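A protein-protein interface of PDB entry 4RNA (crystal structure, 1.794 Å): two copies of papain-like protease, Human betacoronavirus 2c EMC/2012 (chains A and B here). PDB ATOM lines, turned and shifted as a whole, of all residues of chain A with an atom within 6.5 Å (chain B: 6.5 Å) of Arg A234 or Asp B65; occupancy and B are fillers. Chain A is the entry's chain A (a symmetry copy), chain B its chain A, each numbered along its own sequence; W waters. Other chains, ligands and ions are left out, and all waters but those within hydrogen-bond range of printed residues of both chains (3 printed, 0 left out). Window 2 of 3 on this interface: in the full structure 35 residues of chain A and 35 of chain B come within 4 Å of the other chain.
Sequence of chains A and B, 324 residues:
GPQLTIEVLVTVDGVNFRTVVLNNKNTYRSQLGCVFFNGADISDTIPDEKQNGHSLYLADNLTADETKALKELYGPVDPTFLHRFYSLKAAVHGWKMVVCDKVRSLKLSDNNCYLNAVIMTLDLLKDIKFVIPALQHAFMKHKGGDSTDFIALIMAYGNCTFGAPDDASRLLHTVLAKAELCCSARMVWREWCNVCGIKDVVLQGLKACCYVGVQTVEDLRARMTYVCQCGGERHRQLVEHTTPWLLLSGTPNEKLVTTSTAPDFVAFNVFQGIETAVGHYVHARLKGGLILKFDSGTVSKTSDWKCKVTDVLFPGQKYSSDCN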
ATOM      1  N   GLU A 191     -16.129 -27.475  32.708  1.00  0.00           N
ATOM      2  CA  GLU A 191     -16.044 -26.181  32.049  1.00  0.00           C
ATOM      3  C   GLU A 191     -15.236 -25.246  32.990  1.00  0.00           C
ATOM      4  O   GLU A 191     -15.517 -25.159  34.200  1.00  0.00           O
ATOM      5  CB  GLU A 191     -17.458 -25.652  31.781  1.00  0.00           C
ATOM      6  CG  GLU A 191     -18.145 -26.440  30.685  1.00  0.00           C
ATOM      7  CD  GLU A 191     -19.489 -25.866  30.215  1.00  0.00           C
ATOM      8  OE1 GLU A 191     -19.988 -24.874  30.798  1.00  0.00           O
ATOM      9  OE2 GLU A 191     -20.048 -26.430  29.229  1.00  0.00           O
ATOM     10  N   TRP A 192     -14.225 -24.564  32.457  1.00  0.00           N
ATOM     11  CA  TRP A 192     -13.455 -23.677  33.354  1.00  0.00           C
ATOM     12  C   TRP A 192     -12.859 -22.471  32.696  1.00  0.00           C
ATOM     13  O   TRP A 192     -12.622 -22.427  31.463  1.00  0.00           O
ATOM     14  CB  TRP A 192     -12.399 -24.456  34.164  1.00  0.00           C
ATOM     15  CG  TRP A 192     -11.197 -24.775  33.337  1.00  0.00           C
ATOM     16  CD1 TRP A 192      -9.965 -24.091  33.305  1.00  0.00           C
ATOM     17  CD2 TRP A 192     -11.079 -25.837  32.320  1.00  0.00           C
ATOM     18  NE1 TRP A 192      -9.114 -24.652  32.377  1.00  0.00           N
ATOM     19  CE2 TRP A 192      -9.723 -25.701  31.742  1.00  0.00           C
ATOM     20  CE3 TRP A 192     -11.941 -26.830  31.821  1.00  0.00           C
ATOM     21  CZ2 TRP A 192      -9.264 -26.549  30.726  1.00  0.00           C
ATOM     22  CZ3 TRP A 192     -11.484 -27.685  30.791  1.00  0.00           C
ATOM     23  CH2 TRP A 192     -10.158 -27.586  30.290  1.00  0.00           C
ATOM     24  N   CYS A 193     -12.663 -21.473  33.548  1.00  0.00           N
ATOM     25  CA  CYS A 193     -11.834 -20.315  33.299  1.00  0.00           C
ATOM     26  C   CYS A 193     -10.881 -20.163  34.513  1.00  0.00           C
ATOM     27  O   CYS A 193     -11.315 -20.274  35.654  1.00  0.00           O
ATOM     28  CB  CYS A 193     -12.705 -19.064  33.231  1.00  0.00           C
ATOM     29  SG  CYS A 193     -11.759 -17.506  33.181  1.00  0.00           S
ATOM     30  N   LYS A 199     -17.001 -25.270  36.625  1.00  0.00           N
ATOM     31  CA  LYS A 199     -18.295 -25.952  36.757  1.00  0.00           C
ATOM     32  C   LYS A 199     -18.201 -27.361  36.173  1.00  0.00           C
ATOM     33  O   LYS A 199     -17.806 -27.503  34.997  1.00  0.00           O
ATOM     34  CB  LYS A 199     -19.401 -25.213  35.996  1.00  0.00           C
ATOM     35  CG  LYS A 199     -20.813 -25.703  36.324  1.00  0.00           C
ATOM     36  CD  LYS A 199     -20.979 -25.720  37.854  1.00  0.00           C
ATOM     37  CE  LYS A 199     -22.388 -26.072  38.334  1.00  0.00           C
ATOM     38  NZ  LYS A 199     -22.680 -27.521  38.166  1.00  0.00           N
ATOM     39  N   MET A 224     -12.239 -27.866  24.092  1.00  0.00           N
ATOM     40  CA  MET A 224     -12.778 -26.734  23.317  1.00  0.00           C
ATOM     41  C   MET A 224     -12.627 -25.482  24.140  1.00  0.00           C
ATOM     42  O   MET A 224     -12.771 -25.506  25.407  1.00  0.00           O
ATOM     43  CB  MET A 224     -14.270 -26.903  22.951  1.00  0.00           C
ATOM     44  CG  MET A 224     -14.859 -25.657  22.265  1.00  0.00           C
ATOM     45  SD  MET A 224     -16.636 -25.701  21.933  1.00  0.00           S
ATOM     46  CE  MET A 224     -17.281 -25.730  23.612  1.00  0.00           C
ATOM     47  N   THR A 225     -12.394 -24.384  23.428  1.00  0.00           N
ATOM     48  CA  THR A 225     -12.115 -23.105  24.048  1.00  0.00           C
ATOM     49  C   THR A 225     -12.923 -21.976  23.365  1.00  0.00           C
ATOM     50  O   THR A 225     -13.031 -21.916  22.169  1.00  0.00           O
ATOM     51  CB  THR A 225     -10.577 -22.821  23.957  1.00  0.00           C
ATOM     52  OG1 THR A 225      -9.843 -23.811  24.721  1.00  0.00           O
ATOM     53  CG2 THR A 225     -10.237 -21.363  24.394  1.00  0.00           C
ATOM     54  N   TYR A 226     -13.476 -21.044  24.127  1.00  0.00           N
ATOM     55  CA  TYR A 226     -14.072 -19.867  23.429  1.00  0.00           C
ATOM     56  C   TYR A 226     -13.996 -18.681  24.448  1.00  0.00           C
ATOM     57  O   TYR A 226     -13.373 -18.849  25.527  1.00  0.00           O
ATOM     58  CB  TYR A 226     -15.510 -20.199  22.943  1.00  0.00           C
ATOM     59  CG  TYR A 226     -16.366 -20.728  24.078  1.00  0.00           C
ATOM     60  CD1 TYR A 226     -16.290 -22.098  24.481  1.00  0.00           C
ATOM     61  CD2 TYR A 226     -17.229 -19.874  24.758  1.00  0.00           C
ATOM     62  CE1 TYR A 226     -17.061 -22.565  25.552  1.00  0.00           C
ATOM     63  CE2 TYR A 226     -17.980 -20.325  25.831  1.00  0.00           C
ATOM     64  CZ  TYR A 226     -17.898 -21.670  26.217  1.00  0.00           C
ATOM     65  OH  TYR A 226     -18.700 -22.070  27.264  1.00  0.00           O
ATOM     66  N   VAL A 227     -14.598 -17.528  24.108  1.00  0.00           N
ATOM     67  CA  VAL A 227     -14.420 -16.291  24.883  1.00  0.00           C
ATOM     68  C   VAL A 227     -15.147 -16.501  26.182  1.00  0.00           C
ATOM     69  O   VAL A 227     -16.268 -17.068  26.194  1.00  0.00           O
ATOM     70  CB  VAL A 227     -14.923 -15.015  24.118  1.00  0.00           C
ATOM     71  CG1 VAL A 227     -14.948 -13.805  25.045  1.00  0.00           C
ATOM     72  CG2 VAL A 227     -14.044 -14.766  22.888  1.00  0.00           C
ATOM     73  N   CYS A 228     -14.471 -16.141  27.265  1.00  0.00           N
ATOM     74  CA  CYS A 228     -15.104 -16.132  28.588  1.00  0.00           C
ATOM     75  C   CYS A 228     -15.797 -14.779  28.807  1.00  0.00           C
ATOM     76  O   CYS A 228     -15.377 -13.775  28.220  1.00  0.00           O
ATOM     77  CB  CYS A 228     -14.135 -16.433  29.715  1.00  0.00           C
ATOM     78  SG  CYS A 228     -15.140 -16.641  31.208  1.00  0.00           S
ATOM     79  N   GLN A 229     -16.861 -14.786  29.613  1.00  0.00           N
ATOM     80  CA  GLN A 229     -17.532 -13.547  30.024  1.00  0.00           C
ATOM     81  C   GLN A 229     -16.619 -12.547  30.790  1.00  0.00           C
ATOM     82  O   GLN A 229     -16.931 -11.369  30.864  1.00  0.00           O
ATOM     83  CB  GLN A 229     -18.763 -13.858  30.877  1.00  0.00           C
ATOM     84  CG  GLN A 229     -18.495 -14.637  32.150  1.00  0.00           C
ATOM     85  CD  GLN A 229     -18.466 -16.180  31.983  1.00  0.00           C
ATOM     86  OE1 GLN A 229     -18.595 -16.785  30.840  1.00  0.00           O
ATOM     87  NE2 GLN A 229     -18.268 -16.844  33.136  1.00  0.00           N
ATOM     88  N   GLY A 232     -11.610 -13.076  29.109  1.00  0.00           N
ATOM     89  CA  GLY A 232     -10.553 -14.056  28.838  1.00  0.00           C
ATOM     90  C   GLY A 232     -11.047 -15.237  27.998  1.00  0.00           C
ATOM     91  O   GLY A 232     -11.818 -15.053  27.026  1.00  0.00           O
ATOM     92  N   GLU A 233     -10.595 -16.439  28.381  1.00  0.00           N
ATOM     93  CA  GLU A 233     -10.847 -17.693  27.655  1.00  0.00           C
ATOM     94  C   GLU A 233     -11.515 -18.649  28.593  1.00  0.00           C
ATOM     95  O   GLU A 233     -11.251 -18.631  29.802  1.00  0.00           O
ATOM     96  CB  GLU A 233      -9.539 -18.370  27.279  1.00  0.00           C
ATOM     97  CG  GLU A 233      -9.049 -18.034  25.898  1.00  0.00           C
ATOM     98  CD  GLU A 233      -7.701 -18.708  25.596  1.00  0.00           C
ATOM     99  OE1 GLU A 233      -7.261 -18.603  24.429  1.00  0.00           O
ATOM    100  OE2 GLU A 233      -7.091 -19.361  26.501  1.00  0.00           O
ATOM    101  N   ARG A 234     -12.356 -19.501  28.011  1.00  0.00           N
ATOM    102  CA  ARG A 234     -13.210 -20.428  28.740  1.00  0.00           C
ATOM    103  C   ARG A 234     -12.980 -21.769  28.033  1.00  0.00           C
ATOM    104  O   ARG A 234     -12.899 -21.790  26.837  1.00  0.00           O
ATOM    105  CB  ARG A 234     -14.660 -20.023  28.437  1.00  0.00           C
ATOM    106  CG  ARG A 234     -15.473 -19.660  29.609  1.00  0.00           C
ATOM    107  CD  ARG A 234     -16.910 -19.556  29.158  1.00  0.00           C
ATOM    108  NE  ARG A 234     -17.526 -20.742  29.700  1.00  0.00           N
ATOM    109  CZ  ARG A 234     -18.470 -20.772  30.657  1.00  0.00           C
ATOM    110  NH1 ARG A 234     -19.014 -19.643  31.165  1.00  0.00           N
ATOM    111  NH2 ARG A 234     -18.945 -21.949  31.059  1.00  0.00           N
ATOM    112  N   HIS A 235     -12.877 -22.870  28.760  1.00  0.00           N
ATOM    113  CA  HIS A 235     -12.686 -24.177  28.116  1.00  0.00           C
ATOM    114  C   HIS A 235     -13.734 -25.205  28.487  1.00  0.00           C
ATOM    115  O   HIS A 235     -14.344 -25.145  29.545  1.00  0.00           O
ATOM    116  CB  HIS A 235     -11.340 -24.763  28.556  1.00  0.00           C
ATOM    117  CG  HIS A 235     -10.203 -23.817  28.399  1.00  0.00           C
ATOM    118  ND1 HIS A 235      -9.599 -23.612  27.198  1.00  0.00           N
ATOM    119  CD2 HIS A 235      -9.587 -22.970  29.311  1.00  0.00           C
ATOM    120  CE1 HIS A 235      -8.593 -22.702  27.334  1.00  0.00           C
ATOM    121  NE2 HIS A 235      -8.601 -22.276  28.629  1.00  0.00           N
ATOM    122  N   ARG A 236     -13.957 -26.186  27.640  1.00  0.00           N
ATOM    123  CA  ARG A 236     -14.862 -27.298  27.953  1.00  0.00           C
ATOM    124  C   ARG A 236     -14.112 -28.597  27.643  1.00  0.00           C
ATOM    125  O   ARG A 236     -13.594 -28.750  26.492  1.00  0.00           O
ATOM    126  CB  ARG A 236     -16.133 -27.158  27.068  1.00  0.00           C
ATOM    127  CG  ARG A 236     -17.009 -28.394  26.873  1.00  0.00           C
ATOM    128  CD  ARG A 236     -18.401 -27.999  26.339  1.00  0.00           C
ATOM    129  NE  ARG A 236     -19.328 -29.135  26.211  1.00  0.00           N
ATOM    130  CZ  ARG A 236     -20.090 -29.615  27.188  1.00  0.00           C
ATOM    131  NH1 ARG A 236     -20.094 -29.053  28.405  1.00  0.00           N
ATOM    132  NH2 ARG A 236     -20.882 -30.654  26.940  1.00  0.00           N
ATOM    133  N   VAL B  12     -27.996 -20.966  19.896  1.00  0.00           N
ATOM    134  CA  VAL B  12     -29.067 -21.939  19.604  1.00  0.00           C
ATOM    135  C   VAL B  12     -30.474 -21.340  19.702  1.00  0.00           C
ATOM    136  O   VAL B  12     -31.497 -21.990  19.356  1.00  0.00           O
ATOM    137  CB  VAL B  12     -29.005 -23.195  20.493  1.00  0.00           C
ATOM    138  CG1 VAL B  12     -27.652 -23.863  20.454  1.00  0.00           C
ATOM    139  CG2 VAL B  12     -29.429 -22.899  21.973  1.00  0.00           C
ATOM    140  N   LEU B  62     -23.237 -28.739  22.134  1.00  0.00           N
ATOM    141  CA  LEU B  62     -23.636 -27.503  22.697  1.00  0.00           C
ATOM    142  C   LEU B  62     -22.970 -27.568  24.073  1.00  0.00           C
ATOM    143  O   LEU B  62     -22.775 -28.677  24.613  1.00  0.00           O
ATOM    144  CB  LEU B  62     -25.184 -27.473  22.910  1.00  0.00           C
ATOM    145  CG  LEU B  62     -26.264 -27.704  21.834  1.00  0.00           C
ATOM    146  CD1 LEU B  62     -27.637 -27.217  22.324  1.00  0.00           C
ATOM    147  CD2 LEU B  62     -25.958 -27.252  20.395  1.00  0.00           C
ATOM    148  N   THR B  63     -22.642 -26.397  24.572  1.00  0.00           N
ATOM    149  CA  THR B  63     -22.141 -26.184  25.938  1.00  0.00           C
ATOM    150  C   THR B  63     -23.265 -26.405  26.921  1.00  0.00           C
ATOM    151  O   THR B  63     -24.448 -26.535  26.544  1.00  0.00           O
ATOM    152  CB  THR B  63     -21.651 -24.740  26.076  1.00  0.00           C
ATOM    153  OG1 THR B  63     -22.761 -23.857  25.809  1.00  0.00           O
ATOM    154  CG2 THR B  63     -20.548 -24.411  25.026  1.00  0.00           C
ATOM    155  N   ALA B  64     -22.922 -26.479  28.205  1.00  0.00           N
ATOM    156  CA  ALA B  64     -23.914 -26.554  29.192  1.00  0.00           C
ATOM    157  C   ALA B  64     -24.879 -25.379  29.110  1.00  0.00           C
ATOM    158  O   ALA B  64     -26.070 -25.605  29.291  1.00  0.00           O
ATOM    159  CB  ALA B  64     -23.267 -26.608  30.583  1.00  0.00           C
ATOM    160  N   ASP B  65     -24.393 -24.154  28.867  1.00  0.00           N
ATOM    161  CA  ASP B  65     -25.286 -22.983  28.831  1.00  0.00           C
ATOM    162  C   ASP B  65     -26.252 -23.147  27.670  1.00  0.00           C
ATOM    163  O   ASP B  65     -27.432 -22.803  27.782  1.00  0.00           O
ATOM    164  CB  ASP B  65     -24.568 -21.629  28.699  1.00  0.00           C
ATOM    165  CG  ASP B  65     -23.723 -21.258  29.966  1.00  0.00           C
ATOM    166  OD1 ASP B  65     -24.248 -21.467  31.036  1.00  0.00           O
ATOM    167  OD2 ASP B  65     -22.545 -20.786  29.884  1.00  0.00           O
ATOM    168  N   GLU B  66     -25.728 -23.612  26.532  1.00  0.00           N
ATOM    169  CA  GLU B  66     -26.595 -23.739  25.373  1.00  0.00           C
ATOM    170  C   GLU B  66     -27.665 -24.824  25.565  1.00  0.00           C
ATOM    171  O   GLU B  66     -28.796 -24.654  25.103  1.00  0.00           O
ATOM    172  CB  GLU B  66     -25.770 -24.012  24.123  1.00  0.00           C
ATOM    173  CG  GLU B  66     -25.022 -22.765  23.692  1.00  0.00           C
ATOM    174  CD  GLU B  66     -23.864 -23.075  22.743  1.00  0.00           C
ATOM    175  OE1 GLU B  66     -23.363 -24.222  22.785  1.00  0.00           O
ATOM    176  OE2 GLU B  66     -23.420 -22.122  22.014  1.00  0.00           O
ATOM    177  N   THR B  67     -27.291 -25.925  26.225  1.00  0.00           N
ATOM    178  CA  THR B  67     -28.226 -26.986  26.552  1.00  0.00           C
ATOM    179  C   THR B  67     -29.420 -26.454  27.363  1.00  0.00           C
ATOM    180  O   THR B  67     -30.605 -26.741  27.081  1.00  0.00           O
ATOM    181  CB  THR B  67     -27.494 -28.103  27.325  1.00  0.00           C
ATOM    182  OG1 THR B  67     -26.634 -28.758  26.387  1.00  0.00           O
ATOM    183  CG2 THR B  67     -28.441 -29.063  27.848  1.00  0.00           C
ATOM    184  N   LYS B  68     -29.099 -25.633  28.352  1.00  0.00           N
ATOM    185  CA  LYS B  68     -30.139 -24.968  29.117  1.00  0.00           C
ATOM    186  C   LYS B  68     -30.959 -23.927  28.342  1.00  0.00           C
ATOM    187  O   LYS B  68     -32.166 -23.841  28.548  1.00  0.00           O
ATOM    188  CB  LYS B  68     -29.503 -24.350  30.361  1.00  0.00           C
ATOM    189  CG  LYS B  68     -30.484 -23.638  31.270  1.00  0.00           C
ATOM    190  CD  LYS B  68     -29.785 -23.340  32.592  1.00  0.00           C
ATOM    191  CE  LYS B  68     -30.259 -22.048  33.223  1.00  0.00           C
ATOM    192  NZ  LYS B  68     -29.188 -21.562  34.138  1.00  0.00           N
ATOM    193  N   ALA B  69     -30.313 -23.129  27.470  1.00  0.00           N
ATOM    194  CA  ALA B  69     -31.043 -22.208  26.611  1.00  0.00           C
ATOM    195  C   ALA B  69     -31.974 -22.986  25.670  1.00  0.00           C
ATOM    196  O   ALA B  69     -33.136 -22.588  25.444  1.00  0.00           O
ATOM    197  CB  ALA B  69     -30.094 -21.324  25.820  1.00  0.00           C
ATOM    198  N   LEU B  70     -31.459 -24.060  25.101  1.00  0.00           N
ATOM    199  CA  LEU B  70     -32.264 -24.973  24.276  1.00  0.00           C
ATOM    200  C   LEU B  70     -33.541 -25.433  25.056  1.00  0.00           C
ATOM    201  O   LEU B  70     -34.672 -25.222  24.610  1.00  0.00           O
ATOM    202  CB  LEU B  70     -31.416 -26.199  23.888  1.00  0.00           C
ATOM    203  CG  LEU B  70     -32.138 -27.289  23.099  1.00  0.00           C
ATOM    204  CD1 LEU B  70     -32.330 -26.648  21.754  1.00  0.00           C
ATOM    205  CD2 LEU B  70     -31.332 -28.579  22.901  1.00  0.00           C
HETATM  206  O   HOH W   1     -21.567 -23.466  29.290  1.00  0.00           O
HETATM  207  O   HOH W   2     -20.914 -20.108  27.918  1.00  0.00           O
HETATM  208  O   HOH W   3     -21.501 -20.476  32.193  1.00  0.00           O
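OD2 of Asp B65 lies within salt-bridge range of NH1 of Arg A234, at 3.9 Å. The side-chain carboxylate (OE2) of Glu A191 lies within hydrogen-bond range of the backbone NH (N) of Ala B64, at 3.1 Å.
The backbone carbonyl oxygen (O) of Met A224 lies within hydrogen-bond range of the backbone NH (N) of Arg A236, at 2.6 Å. The side-chain hydroxyl (OG1) of Thr B63 lies close to the backbone NH (N) of Asp B65, at 3.5 Å. The side-chain carboxylate of Glu A191 lies within salt-bridge range of the guanidinium group of Arg A234 (3.1 Å). The backbone carbonyl oxygen of Thr B63 is in hydrogen-bond range of the side-chain hydroxyl of Thr B67, 3.1 Å away. O of Tyr A226 sits at hydrogen-bond distance from N of Arg A234. The backbone NH of Thr B63 is in hydrogen-bond range of the side-chain carboxylate of Glu B66, at 2.9 Å.
Among the printed residues, pairs that only touch across the chains: Glu A191 with Thr B63 (3.9 Å), Met A224 with Thr B63 (3.8 Å), Tyr A226 with Thr B63 (3.7 Å), Arg A236 with Leu B62 (3.6 Å) and Arg A236 with Ala B64 (3.8 Å).
Arg A234 touches just one residue of chain B: Asp B65 (3.9 Å). Asp B65 touches just one residue of chain A: Arg A234 (3.9 Å). Of the printed residues of chain B, Glu A191 touches Thr B63 and Ala B64. Of the printed residues of chain B, Tyr A226 touches Thr B63 (3.7 Å). Printed residues of chain B within 4 Å of Met A224: Thr B63 (3.8 Å). Printed residues of chain B within 4 Å of Arg A236: Leu B62 and Ala B64. Of the printed residues of chain A, Ala B64 touches Glu A191 and Arg A236. Val A227 touches none of the printed residues of chain B. The nearest residue of chain A that does not touch Asp B65 is Tyr A226 (4.8 Å). The nearest printed residue of chain B that does not touch Met A224 is Leu B62 (6.0 Å).
Of the 10 printed residues of chain B, 4 touch a printed residue of chain A. Hydrophobic or aromatic side chains of chain B that line the printed part of chain A: Ala B64.
No position is printed for both chains.
Water W3 bridges OD2 of Asp B65 and NH1 of Arg A234. Water W1 lies within hydrogen-bond range of the side-chain carboxylate (OE1) of Glu A191 (2.6 Å), the side-chain carboxylate (OD2) of Asp B65 (2.9 Å) and the backbone NH (N) of Ala B64 (3.5 Å). Water W2 lies within hydrogen-bond range of the side-chain carboxylate (OD2) of Asp B65 (2.6 Å) and the side-chain hydroxyl (OH) of Tyr A226 (3.0 Å).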
